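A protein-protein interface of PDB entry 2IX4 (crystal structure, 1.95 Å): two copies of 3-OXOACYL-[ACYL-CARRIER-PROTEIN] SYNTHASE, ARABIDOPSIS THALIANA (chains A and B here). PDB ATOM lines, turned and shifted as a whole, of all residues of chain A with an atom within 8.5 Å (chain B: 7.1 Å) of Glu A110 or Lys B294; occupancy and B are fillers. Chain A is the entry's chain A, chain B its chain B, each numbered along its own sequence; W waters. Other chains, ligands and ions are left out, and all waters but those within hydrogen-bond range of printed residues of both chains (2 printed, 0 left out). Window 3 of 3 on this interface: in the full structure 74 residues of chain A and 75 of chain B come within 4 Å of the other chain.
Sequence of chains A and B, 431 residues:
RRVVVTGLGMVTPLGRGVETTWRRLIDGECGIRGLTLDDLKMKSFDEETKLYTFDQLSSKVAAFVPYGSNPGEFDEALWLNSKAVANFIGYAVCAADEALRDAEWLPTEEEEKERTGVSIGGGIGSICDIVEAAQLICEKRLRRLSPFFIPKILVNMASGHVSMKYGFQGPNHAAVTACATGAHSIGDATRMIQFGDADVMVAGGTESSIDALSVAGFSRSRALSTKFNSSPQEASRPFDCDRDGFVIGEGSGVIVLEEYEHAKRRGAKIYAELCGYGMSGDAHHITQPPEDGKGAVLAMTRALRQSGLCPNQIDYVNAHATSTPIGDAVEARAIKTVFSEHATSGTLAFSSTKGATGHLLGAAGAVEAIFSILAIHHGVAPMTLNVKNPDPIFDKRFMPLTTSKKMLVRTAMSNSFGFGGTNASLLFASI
Of chain B, only Lys B294 comes within 4 Å of Glu A110. Lys B294 touches three residues of chain A. No residue of chain A comes within 4 Å of Gly B295. Printed residues of chain A within 4 Å of Gly B281: Gln A169 (3.4 Å) and Gly A170 (3.2 Å). Of the printed residues of chain A, Arg B302 touches Glu A114 (2.9 Å), Gln A169 (2.9 Å) and Gly A170 (3.7 Å). Printed residues of chain B within 4 Å of Gln A169: Ser B280, Gly B281, Lys B294 and Arg B302. Asp B292 touches none of the printed residues of chain A. Pro B290 touches none of the printed residues of chain A. The nearest printed residue of chain B that does not touch Glu A110 is Leu B298 (7.0 Å). The nearest printed residue of chain A that does not touch Lys B294 is Glu A111 (6.8 Å). The nearest printed residue of chain A that does not touch Gly B281 is Phe A168 (4.4 Å).
Water W2 bridges NH1 of Arg A115 (2.8 Å) and NE of Arg B302 (3.3 Å). Water W1 lies within hydrogen-bond range of O of Gly B281 (2.8 Å), OE1 of Gln A169 (2.9 Å) and N of Gly B295 (3.5 Å).
NE2 of Gln A169 lies within hydrogen-bond range of OE1 of Glu A110 (2.8 Å). O of Lys A113 sits at hydrogen-bond distance from N of Gln A169. The backbone carbonyl oxygen of Glu A114 sits close to the backbone NH of Gly A170 (3.4 Å). O of Thr A116 is in hydrogen-bond range of N of Gln A169. The backbone carbonyl oxygen of Thr A116 is in hydrogen-bond range of the backbone NH of Gly A170, 2.8 Å away. N of Asn B423 lies within hydrogen-bond range of O of Ser B280, at 3.0 Å.
Among the printed residues, merely in contact across the chains: Gln A169 with Ser B280, Gly A170 with Ser B280 and Gly A170 with Arg B302.
Of the 19 printed residues of chain B, 4 touch a printed residue of chain A. Among the printed residues, 10 pairs touch across the chains. Among the printed residues, Asp or Glu carboxylates within 4 Å of a Lys or Arg side-chain nitrogen of the other chain: Glu A110 with Lys B294 (2.9 Å) and Glu A114 with Lys B294 (2.7 Å).
No position is printed for both chains. Of the 10 pairs that touch across the chains among the printed residues, none has its exchanged pair printed and touching as well.
OE1 of Glu A110 is in salt-bridge range of NZ of Lys B294 (2.9 Å). NZ of Lys B294 lies within salt-bridge range of OE2 of Glu A114 (2.7 Å). The backbone carbonyl oxygen (O) of Glu A114 is in hydrogen-bond range of the guanidinium group (NH2) of Arg B302 (2.9 Å). The backbone carbonyl oxygen (O) of Gln A169 lies within hydrogen-bond range of the backbone NH (N) of Gly B281, at 3.4 Å. The side-chain amide oxygen of Gln A169 sits at hydrogen-bond distance from the side-chain amino group of Lys B294, 2.8 Å away. The backbone carbonyl oxygen of Gln A169 lies within hydrogen-bond range of the guanidinium group of Arg B302 (2.9 Å). The backbone carbonyl oxygen (O) of Gly A170 lies within hydrogen-bond range of the backbone NH (N) of Gly B281, 3.2 Å away.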
ATOM      1  N   PRO A 107      19.627  31.393  22.501  1.00  0.00           N
ATOM      2  CA  PRO A 107      18.560  31.359  21.500  1.00  0.00           C
ATOM      3  C   PRO A 107      17.610  30.178  21.679  1.00  0.00           C
ATOM      4  O   PRO A 107      18.028  29.093  22.085  1.00  0.00           O
ATOM      5  CB  PRO A 107      19.320  31.238  20.177  1.00  0.00           C
ATOM      6  CG  PRO A 107      20.623  30.631  20.535  1.00  0.00           C
ATOM      7  CD  PRO A 107      20.952  31.175  21.891  1.00  0.00           C
ATOM      8  N   THR A 108      16.337  30.411  21.386  1.00  0.00           N
ATOM      9  CA  THR A 108      15.329  29.360  21.418  1.00  0.00           C
ATOM     10  C   THR A 108      15.001  28.884  20.003  1.00  0.00           C
ATOM     11  O   THR A 108      14.530  27.761  19.812  1.00  0.00           O
ATOM     12  CB  THR A 108      14.039  29.849  22.097  1.00  0.00           C
ATOM     13  OG1 THR A 108      13.585  31.041  21.446  1.00  0.00           O
ATOM     14  CG2 THR A 108      14.285  30.147  23.567  1.00  0.00           C
ATOM     15  N   GLU A 109      15.253  29.745  19.019  1.00  0.00           N
ATOM     16  CA  GLU A 109      14.924  29.460  17.626  1.00  0.00           C
ATOM     17  C   GLU A 109      15.978  28.556  17.004  1.00  0.00           C
ATOM     18  O   GLU A 109      17.175  28.764  17.208  1.00  0.00           O
ATOM     19  CB  GLU A 109      14.801  30.761  16.828  1.00  0.00           C
ATOM     20  CG  GLU A 109      13.616  31.643  17.237  1.00  0.00           C
ATOM     21  CD  GLU A 109      12.270  31.072  16.814  1.00  0.00           C
ATOM     22  OE1 GLU A 109      11.286  31.238  17.567  1.00  0.00           O
ATOM     23  OE2 GLU A 109      12.189  30.458  15.726  1.00  0.00           O
ATOM     24  N   GLU A 110      15.523  27.556  16.248  1.00  0.00           N
ATOM     25  CA  GLU A 110      16.424  26.583  15.620  1.00  0.00           C
ATOM     26  C   GLU A 110      17.379  27.238  14.626  1.00  0.00           C
ATOM     27  O   GLU A 110      18.529  26.818  14.500  1.00  0.00           O
ATOM     28  CB  GLU A 110      15.641  25.447  14.948  1.00  0.00           C
ATOM     29  CG  GLU A 110      15.053  24.409  15.917  1.00  0.00           C
ATOM     30  CD  GLU A 110      16.112  23.584  16.644  1.00  0.00           C
ATOM     31  OE1 GLU A 110      17.165  23.270  16.046  1.00  0.00           O
ATOM     32  OE2 GLU A 110      15.886  23.243  17.825  1.00  0.00           O
ATOM     33  N   GLU A 111      16.899  28.274  13.939  1.00  0.00           N
ATOM     34  CA  GLU A 111      17.713  29.028  12.982  1.00  0.00           C
ATOM     35  C   GLU A 111      18.994  29.602  13.605  1.00  0.00           C
ATOM     36  O   GLU A 111      20.080  29.466  13.033  1.00  0.00           O
ATOM     37  CB  GLU A 111      16.880  30.137  12.331  1.00  0.00           C
ATOM     38  CG  GLU A 111      17.636  30.977  11.309  1.00  0.00           C
ATOM     39  CD  GLU A 111      16.711  31.791  10.427  1.00  0.00           C
ATOM     40  OE1 GLU A 111      16.583  31.448   9.234  1.00  0.00           O
ATOM     41  OE2 GLU A 111      16.101  32.763  10.923  1.00  0.00           O
ATOM     42  N   GLU A 112      18.844  30.230  14.772  1.00  0.00           N
ATOM     43  CA  GLU A 112      19.953  30.842  15.504  1.00  0.00           C
ATOM     44  C   GLU A 112      20.843  29.777  16.146  1.00  0.00           C
ATOM     45  O   GLU A 112      22.070  29.900  16.141  1.00  0.00           O
ATOM     46  CB  GLU A 112      19.425  31.810  16.575  1.00  0.00           C
ATOM     47  CG  GLU A 112      18.553  32.951  16.037  1.00  0.00           C
ATOM     48  CD  GLU A 112      17.981  33.848  17.133  1.00  0.00           C
ATOM     49  OE1 GLU A 112      17.868  35.070  16.895  1.00  0.00           O
ATOM     50  OE2 GLU A 112      17.631  33.344  18.223  1.00  0.00           O
ATOM     51  N   LYS A 113      20.211  28.737  16.689  1.00  0.00           N
ATOM     52  CA  LYS A 113      20.906  27.599  17.314  1.00  0.00           C
ATOM     53  C   LYS A 113      21.822  26.888  16.318  1.00  0.00           C
ATOM     54  O   LYS A 113      22.949  26.518  16.647  1.00  0.00           O
ATOM     55  CB  LYS A 113      19.891  26.590  17.850  1.00  0.00           C
ATOM     56  CG  LYS A 113      19.230  26.954  19.168  1.00  0.00           C
ATOM     57  CD  LYS A 113      18.313  25.818  19.600  1.00  0.00           C
ATOM     58  CE  LYS A 113      17.764  26.020  20.996  1.00  0.00           C
ATOM     59  NZ  LYS A 113      16.988  24.826  21.439  1.00  0.00           N
ATOM     60  N   GLU A 114      21.317  26.708  15.100  1.00  0.00           N
ATOM     61  CA  GLU A 114      22.067  26.079  14.012  1.00  0.00           C
ATOM     62  C   GLU A 114      23.229  26.940  13.527  1.00  0.00           C
ATOM     63  O   GLU A 114      24.190  26.423  12.948  1.00  0.00           O
ATOM     64  CB  GLU A 114      21.134  25.762  12.840  1.00  0.00           C
ATOM     65  CG  GLU A 114      20.210  24.576  13.076  1.00  0.00           C
ATOM     66  CD  GLU A 114      19.175  24.403  11.974  1.00  0.00           C
ATOM     67  OE1 GLU A 114      19.351  24.972  10.873  1.00  0.00           O
ATOM     68  OE2 GLU A 114      18.176  23.694  12.212  1.00  0.00           O
ATOM     69  N   ARG A 115      23.141  28.247  13.764  1.00  0.00           N
ATOM     70  CA  ARG A 115      24.208  29.179  13.385  1.00  0.00           C
ATOM     71  C   ARG A 115      25.202  29.456  14.518  1.00  0.00           C
ATOM     72  O   ARG A 115      26.116  30.269  14.364  1.00  0.00           O
ATOM     73  CB  ARG A 115      23.623  30.488  12.833  1.00  0.00           C
ATOM     74  CG  ARG A 115      22.985  30.360  11.446  1.00  0.00           C
ATOM     75  CD  ARG A 115      23.995  29.881  10.393  1.00  0.00           C
ATOM     76  NE  ARG A 115      24.961  30.914  10.026  1.00  0.00           N
ATOM     77  CZ  ARG A 115      26.043  30.710   9.277  1.00  0.00           C
ATOM     78  NH1 ARG A 115      26.322  29.500   8.812  1.00  0.00           N
ATOM     79  NH2 ARG A 115      26.856  31.720   8.995  1.00  0.00           N
ATOM     80  N   THR A 116      25.021  28.767  15.644  1.00  0.00           N
ATOM     81  CA  THR A 116      25.916  28.881  16.798  1.00  0.00           C
ATOM     82  C   THR A 116      26.722  27.600  16.991  1.00  0.00           C
ATOM     83  O   THR A 116      26.157  26.518  17.129  1.00  0.00           O
ATOM     84  CB  THR A 116      25.129  29.179  18.093  1.00  0.00           C
ATOM     85  OG1 THR A 116      24.271  30.307  17.882  1.00  0.00           O
ATOM     86  CG2 THR A 116      26.083  29.469  19.261  1.00  0.00           C
ATOM     87  N   TYR A 166      22.856  23.789  25.272  1.00  0.00           N
ATOM     88  CA  TYR A 166      22.188  24.955  24.690  1.00  0.00           C
ATOM     89  C   TYR A 166      21.564  24.688  23.317  1.00  0.00           C
ATOM     90  O   TYR A 166      20.885  25.553  22.762  1.00  0.00           O
ATOM     91  CB  TYR A 166      23.159  26.138  24.642  1.00  0.00           C
ATOM     92  CG  TYR A 166      23.786  26.442  25.981  1.00  0.00           C
ATOM     93  CD1 TYR A 166      25.075  26.006  26.284  1.00  0.00           C
ATOM     94  CD2 TYR A 166      23.077  27.136  26.962  1.00  0.00           C
ATOM     95  CE1 TYR A 166      25.652  26.269  27.519  1.00  0.00           C
ATOM     96  CE2 TYR A 166      23.644  27.405  28.201  1.00  0.00           C
ATOM     97  CZ  TYR A 166      24.928  26.968  28.471  1.00  0.00           C
ATOM     98  OH  TYR A 166      25.489  27.227  29.696  1.00  0.00           O
ATOM     99  N   GLY A 167      21.784  23.488  22.786  1.00  0.00           N
ATOM    100  CA  GLY A 167      21.230  23.099  21.493  1.00  0.00           C
ATOM    101  C   GLY A 167      21.973  23.731  20.334  1.00  0.00           C
ATOM    102  O   GLY A 167      21.384  24.002  19.290  1.00  0.00           O
ATOM    103  N   PHE A 168      23.269  23.963  20.520  1.00  0.00           N
ATOM    104  CA  PHE A 168      24.085  24.627  19.507  1.00  0.00           C
ATOM    105  C   PHE A 168      24.522  23.640  18.429  1.00  0.00           C
ATOM    106  O   PHE A 168      25.252  22.683  18.712  1.00  0.00           O
ATOM    107  CB  PHE A 168      25.295  25.327  20.147  1.00  0.00           C
ATOM    108  CG  PHE A 168      24.936  26.507  21.022  1.00  0.00           C
ATOM    109  CD1 PHE A 168      25.809  26.932  22.018  1.00  0.00           C
ATOM    110  CD2 PHE A 168      23.728  27.189  20.856  1.00  0.00           C
ATOM    111  CE1 PHE A 168      25.496  28.023  22.831  1.00  0.00           C
ATOM    112  CE2 PHE A 168      23.401  28.279  21.666  1.00  0.00           C
ATOM    113  CZ  PHE A 168      24.289  28.697  22.656  1.00  0.00           C
ATOM    114  N   GLN A 169      24.076  23.883  17.197  1.00  0.00           N
ATOM    115  CA  GLN A 169      24.252  22.929  16.099  1.00  0.00           C
ATOM    116  C   GLN A 169      25.156  23.438  14.973  1.00  0.00           C
ATOM    117  O   GLN A 169      25.204  22.850  13.888  1.00  0.00           O
ATOM    118  CB  GLN A 169      22.892  22.488  15.552  1.00  0.00           C
ATOM    119  CG  GLN A 169      22.020  21.784  16.582  1.00  0.00           C
ATOM    120  CD  GLN A 169      20.551  21.806  16.216  1.00  0.00           C
ATOM    121  OE1 GLN A 169      20.125  21.130  15.285  1.00  0.00           O
ATOM    122  NE2 GLN A 169      19.767  22.579  16.958  1.00  0.00           N
ATOM    123  N   GLY A 170      25.872  24.528  15.240  1.00  0.00           N
ATOM    124  CA  GLY A 170      26.935  24.989  14.355  1.00  0.00           C
ATOM    125  C   GLY A 170      28.153  24.103  14.530  1.00  0.00           C
ATOM    126  O   GLY A 170      28.065  23.053  15.174  1.00  0.00           O
ATOM    127  N   SER B 280      28.919  20.446  11.860  1.00  0.00           N
ATOM    128  CA  SER B 280      27.711  20.577  12.668  1.00  0.00           C
ATOM    129  C   SER B 280      27.851  19.858  14.004  1.00  0.00           C
ATOM    130  O   SER B 280      28.816  19.128  14.237  1.00  0.00           O
ATOM    131  CB  SER B 280      26.491  20.038  11.915  1.00  0.00           C
ATOM    132  OG  SER B 280      26.505  18.620  11.882  1.00  0.00           O
ATOM    133  N   GLY B 281      26.876  20.085  14.878  1.00  0.00           N
ATOM    134  CA  GLY B 281      26.763  19.354  16.126  1.00  0.00           C
ATOM    135  C   GLY B 281      25.379  18.756  16.242  1.00  0.00           C
ATOM    136  O   GLY B 281      24.389  19.403  15.880  1.00  0.00           O
ATOM    137  N   ASP B 282      25.311  17.515  16.731  1.00  0.00           N
ATOM    138  CA  ASP B 282      24.032  16.849  17.001  1.00  0.00           C
ATOM    139  C   ASP B 282      23.297  17.532  18.146  1.00  0.00           C
ATOM    140  O   ASP B 282      22.065  17.629  18.133  1.00  0.00           O
ATOM    141  CB  ASP B 282      24.242  15.379  17.388  1.00  0.00           C
ATOM    142  CG  ASP B 282      24.728  14.513  16.235  1.00  0.00           C
ATOM    143  OD1 ASP B 282      24.583  14.905  15.055  1.00  0.00           O
ATOM    144  OD2 ASP B 282      25.250  13.411  16.524  1.00  0.00           O
ATOM    145  N   PRO B 290      21.197  11.422  16.946  1.00  0.00           N
ATOM    146  CA  PRO B 290      19.732  11.456  17.006  1.00  0.00           C
ATOM    147  C   PRO B 290      19.122  10.574  15.918  1.00  0.00           C
ATOM    148  O   PRO B 290      19.758  10.337  14.884  1.00  0.00           O
ATOM    149  CB  PRO B 290      19.404  12.929  16.743  1.00  0.00           C
ATOM    150  CG  PRO B 290      20.552  13.432  15.932  1.00  0.00           C
ATOM    151  CD  PRO B 290      21.757  12.688  16.434  1.00  0.00           C
ATOM    152  N   GLU B 291      17.904  10.093  16.155  1.00  0.00           N
ATOM    153  CA  GLU B 291      17.245   9.158  15.244  1.00  0.00           C
ATOM    154  C   GLU B 291      17.157   9.686  13.808  1.00  0.00           C
ATOM    155  O   GLU B 291      17.403   8.940  12.855  1.00  0.00           O
ATOM    156  CB  GLU B 291      15.855   8.791  15.770  1.00  0.00           C
ATOM    157  CG  GLU B 291      15.186   7.642  15.025  1.00  0.00           C
ATOM    158  CD  GLU B 291      13.843   7.251  15.621  1.00  0.00           C
ATOM    159  OE1 GLU B 291      13.079   8.150  16.045  1.00  0.00           O
ATOM    160  OE2 GLU B 291      13.549   6.036  15.655  1.00  0.00           O
ATOM    161  N   ASP B 292      16.822  10.968  13.662  1.00  0.00           N
ATOM    162  CA  ASP B 292      16.635  11.587  12.344  1.00  0.00           C
ATOM    163  C   ASP B 292      17.947  11.964  11.651  1.00  0.00           C
ATOM    164  O   ASP B 292      17.954  12.300  10.465  1.00  0.00           O
ATOM    165  CB  ASP B 292      15.702  12.805  12.437  1.00  0.00           C
ATOM    166  CG  ASP B 292      16.277  13.942  13.277  1.00  0.00           C
ATOM    167  OD1 ASP B 292      17.488  13.939  13.601  1.00  0.00           O
ATOM    168  OD2 ASP B 292      15.500  14.860  13.612  1.00  0.00           O
ATOM    169  N   GLY B 293      19.047  11.916  12.397  1.00  0.00           N
ATOM    170  CA  GLY B 293      20.367  12.241  11.857  1.00  0.00           C
ATOM    171  C   GLY B 293      20.501  13.661  11.336  1.00  0.00           C
ATOM    172  O   GLY B 293      21.199  13.897  10.352  1.00  0.00           O
ATOM    173  N   LYS B 294      19.834  14.604  12.002  1.00  0.00           N
ATOM    174  CA  LYS B 294      19.879  16.018  11.620  1.00  0.00           C
ATOM    175  C   LYS B 294      21.308  16.554  11.529  1.00  0.00           C
ATOM    176  O   LYS B 294      21.641  17.288  10.597  1.00  0.00           O
ATOM    177  CB  LYS B 294      19.058  16.871  12.592  1.00  0.00           C
ATOM    178  CG  LYS B 294      18.871  18.305  12.127  1.00  0.00           C
ATOM    179  CD  LYS B 294      18.188  19.158  13.173  1.00  0.00           C
ATOM    180  CE  LYS B 294      18.236  20.617  12.761  1.00  0.00           C
ATOM    181  NZ  LYS B 294      17.755  21.532  13.839  1.00  0.00           N
ATOM    182  N   GLY B 295      22.145  16.184  12.494  1.00  0.00           N
ATOM    183  CA  GLY B 295      23.541  16.608  12.506  1.00  0.00           C
ATOM    184  C   GLY B 295      24.271  16.200  11.242  1.00  0.00           C
ATOM    185  O   GLY B 295      24.952  17.019  10.619  1.00  0.00           O
ATOM    186  N   ALA B 296      24.116  14.932  10.866  1.00  0.00           N
ATOM    187  CA  ALA B 296      24.692  14.392   9.634  1.00  0.00           C
ATOM    188  C   ALA B 296      24.171  15.120   8.392  1.00  0.00           C
ATOM    189  O   ALA B 296      24.944  15.456   7.497  1.00  0.00           O
ATOM    190  CB  ALA B 296      24.417  12.896   9.533  1.00  0.00           C
ATOM    191  N   VAL B 297      22.862  15.366   8.355  1.00  0.00           N
ATOM    192  CA  VAL B 297      22.234  16.105   7.255  1.00  0.00           C
ATOM    193  C   VAL B 297      22.863  17.494   7.127  1.00  0.00           C
ATOM    194  O   VAL B 297      23.285  17.890   6.033  1.00  0.00           O
ATOM    195  CB  VAL B 297      20.694  16.211   7.436  1.00  0.00           C
ATOM    196  CG1 VAL B 297      20.081  17.189   6.436  1.00  0.00           C
ATOM    197  CG2 VAL B 297      20.043  14.840   7.292  1.00  0.00           C
ATOM    198  N   LEU B 298      22.946  18.204   8.252  1.00  0.00           N
ATOM    199  CA  LEU B 298      23.532  19.544   8.301  1.00  0.00           C
ATOM    200  C   LEU B 298      24.969  19.581   7.799  1.00  0.00           C
ATOM    201  O   LEU B 298      25.316  20.448   7.006  1.00  0.00           O
ATOM    202  CB  LEU B 298      23.444  20.136   9.714  1.00  0.00           C
ATOM    203  CG  LEU B 298      22.076  20.679  10.151  1.00  0.00           C
ATOM    204  CD1 LEU B 298      22.088  20.995  11.632  1.00  0.00           C
ATOM    205  CD2 LEU B 298      21.688  21.912   9.349  1.00  0.00           C
ATOM    206  N   ALA B 299      25.790  18.634   8.246  1.00  0.00           N
ATOM    207  CA  ALA B 299      27.193  18.569   7.832  1.00  0.00           C
ATOM    208  C   ALA B 299      27.334  18.350   6.321  1.00  0.00           C
ATOM    209  O   ALA B 299      28.132  19.025   5.657  1.00  0.00           O
ATOM    210  CB  ALA B 299      27.921  17.481   8.610  1.00  0.00           C
ATOM    211  N   MET B 300      26.549  17.418   5.781  1.00  0.00           N
ATOM    212  CA  MET B 300      26.552  17.129   4.343  1.00  0.00           C
ATOM    213  C   MET B 300      26.024  18.305   3.529  1.00  0.00           C
ATOM    214  O   MET B 300      26.621  18.681   2.523  1.00  0.00           O
ATOM    215  CB  MET B 300      25.748  15.866   4.027  1.00  0.00           C
ATOM    216  CG  MET B 300      26.451  14.576   4.413  1.00  0.00           C
ATOM    217  SD  MET B 300      25.539  13.091   3.959  1.00  0.00           S
ATOM    218  CE  MET B 300      24.294  13.013   5.246  1.00  0.00           C
ATOM    219  N   THR B 301      24.907  18.876   3.974  1.00  0.00           N
ATOM    220  CA  THR B 301      24.304  20.043   3.333  1.00  0.00           C
ATOM    221  C   THR B 301      25.254  21.245   3.315  1.00  0.00           C
ATOM    222  O   THR B 301      25.352  21.955   2.310  1.00  0.00           O
ATOM    223  CB  THR B 301      22.965  20.405   4.014  1.00  0.00           C
ATOM    224  OG1 THR B 301      22.075  19.288   3.900  1.00  0.00           O
ATOM    225  CG2 THR B 301      22.317  21.619   3.362  1.00  0.00           C
ATOM    226  N   ARG B 302      25.972  21.453   4.417  1.00  0.00           N
ATOM    227  CA  ARG B 302      26.913  22.564   4.532  1.00  0.00           C
ATOM    228  C   ARG B 302      28.104  22.437   3.575  1.00  0.00           C
ATOM    229  O   ARG B 302      28.480  23.413   2.930  1.00  0.00           O
ATOM    230  CB  ARG B 302      27.360  22.745   5.988  1.00  0.00           C
ATOM    231  CG  ARG B 302      26.331  23.527   6.811  1.00  0.00           C
ATOM    232  CD  ARG B 302      26.431  23.285   8.309  1.00  0.00           C
ATOM    233  NE  ARG B 302      25.295  23.905   8.994  1.00  0.00           N
ATOM    234  CZ  ARG B 302      25.118  23.935  10.312  1.00  0.00           C
ATOM    235  NH1 ARG B 302      26.003  23.378  11.128  1.00  0.00           N
ATOM    236  NH2 ARG B 302      24.043  24.529  10.814  1.00  0.00           N
ATOM    237  N   VAL B 330      21.126   5.531  11.102  1.00  0.00           N
ATOM    238  CA  VAL B 330      20.914   6.975  11.193  1.00  0.00           C
ATOM    239  C   VAL B 330      21.579   7.688  10.011  1.00  0.00           C
ATOM    240  O   VAL B 330      20.979   8.566   9.388  1.00  0.00           O
ATOM    241  CB  VAL B 330      21.403   7.534  12.566  1.00  0.00           C
ATOM    242  CG1 VAL B 330      21.561   9.042  12.526  1.00  0.00           C
ATOM    243  CG2 VAL B 330      20.436   7.134  13.682  1.00  0.00           C
ATOM    244  N   ALA B 334      20.032   9.749   6.807  1.00  0.00           N
ATOM    245  CA  ALA B 334      20.579  11.070   6.511  1.00  0.00           C
ATOM    246  C   ALA B 334      21.009  11.190   5.051  1.00  0.00           C
ATOM    247  O   ALA B 334      20.747  12.209   4.412  1.00  0.00           O
ATOM    248  CB  ALA B 334      21.734  11.395   7.445  1.00  0.00           C
ATOM    249  N   ASN B 423      30.263  16.554  14.015  1.00  0.00           N
ATOM    250  CA  ASN B 423      30.150  16.048  12.650  1.00  0.00           C
ATOM    251  C   ASN B 423      30.958  16.854  11.657  1.00  0.00           C
ATOM    252  O   ASN B 423      30.974  18.082  11.708  1.00  0.00           O
ATOM    253  CB  ASN B 423      28.688  16.024  12.199  1.00  0.00           C
ATOM    254  CG  ASN B 423      27.782  15.329  13.191  1.00  0.00           C
ATOM    255  OD1 ASN B 423      28.062  14.213  13.629  1.00  0.00           O
ATOM    256  ND2 ASN B 423      26.689  15.985  13.551  1.00  0.00           N
HETATM  257  O   HOH W   1      21.950  18.974  14.557  1.00  0.00           O
HETATM  258  O   HOH W   2      24.942  27.110   8.413  1.00  0.00           O
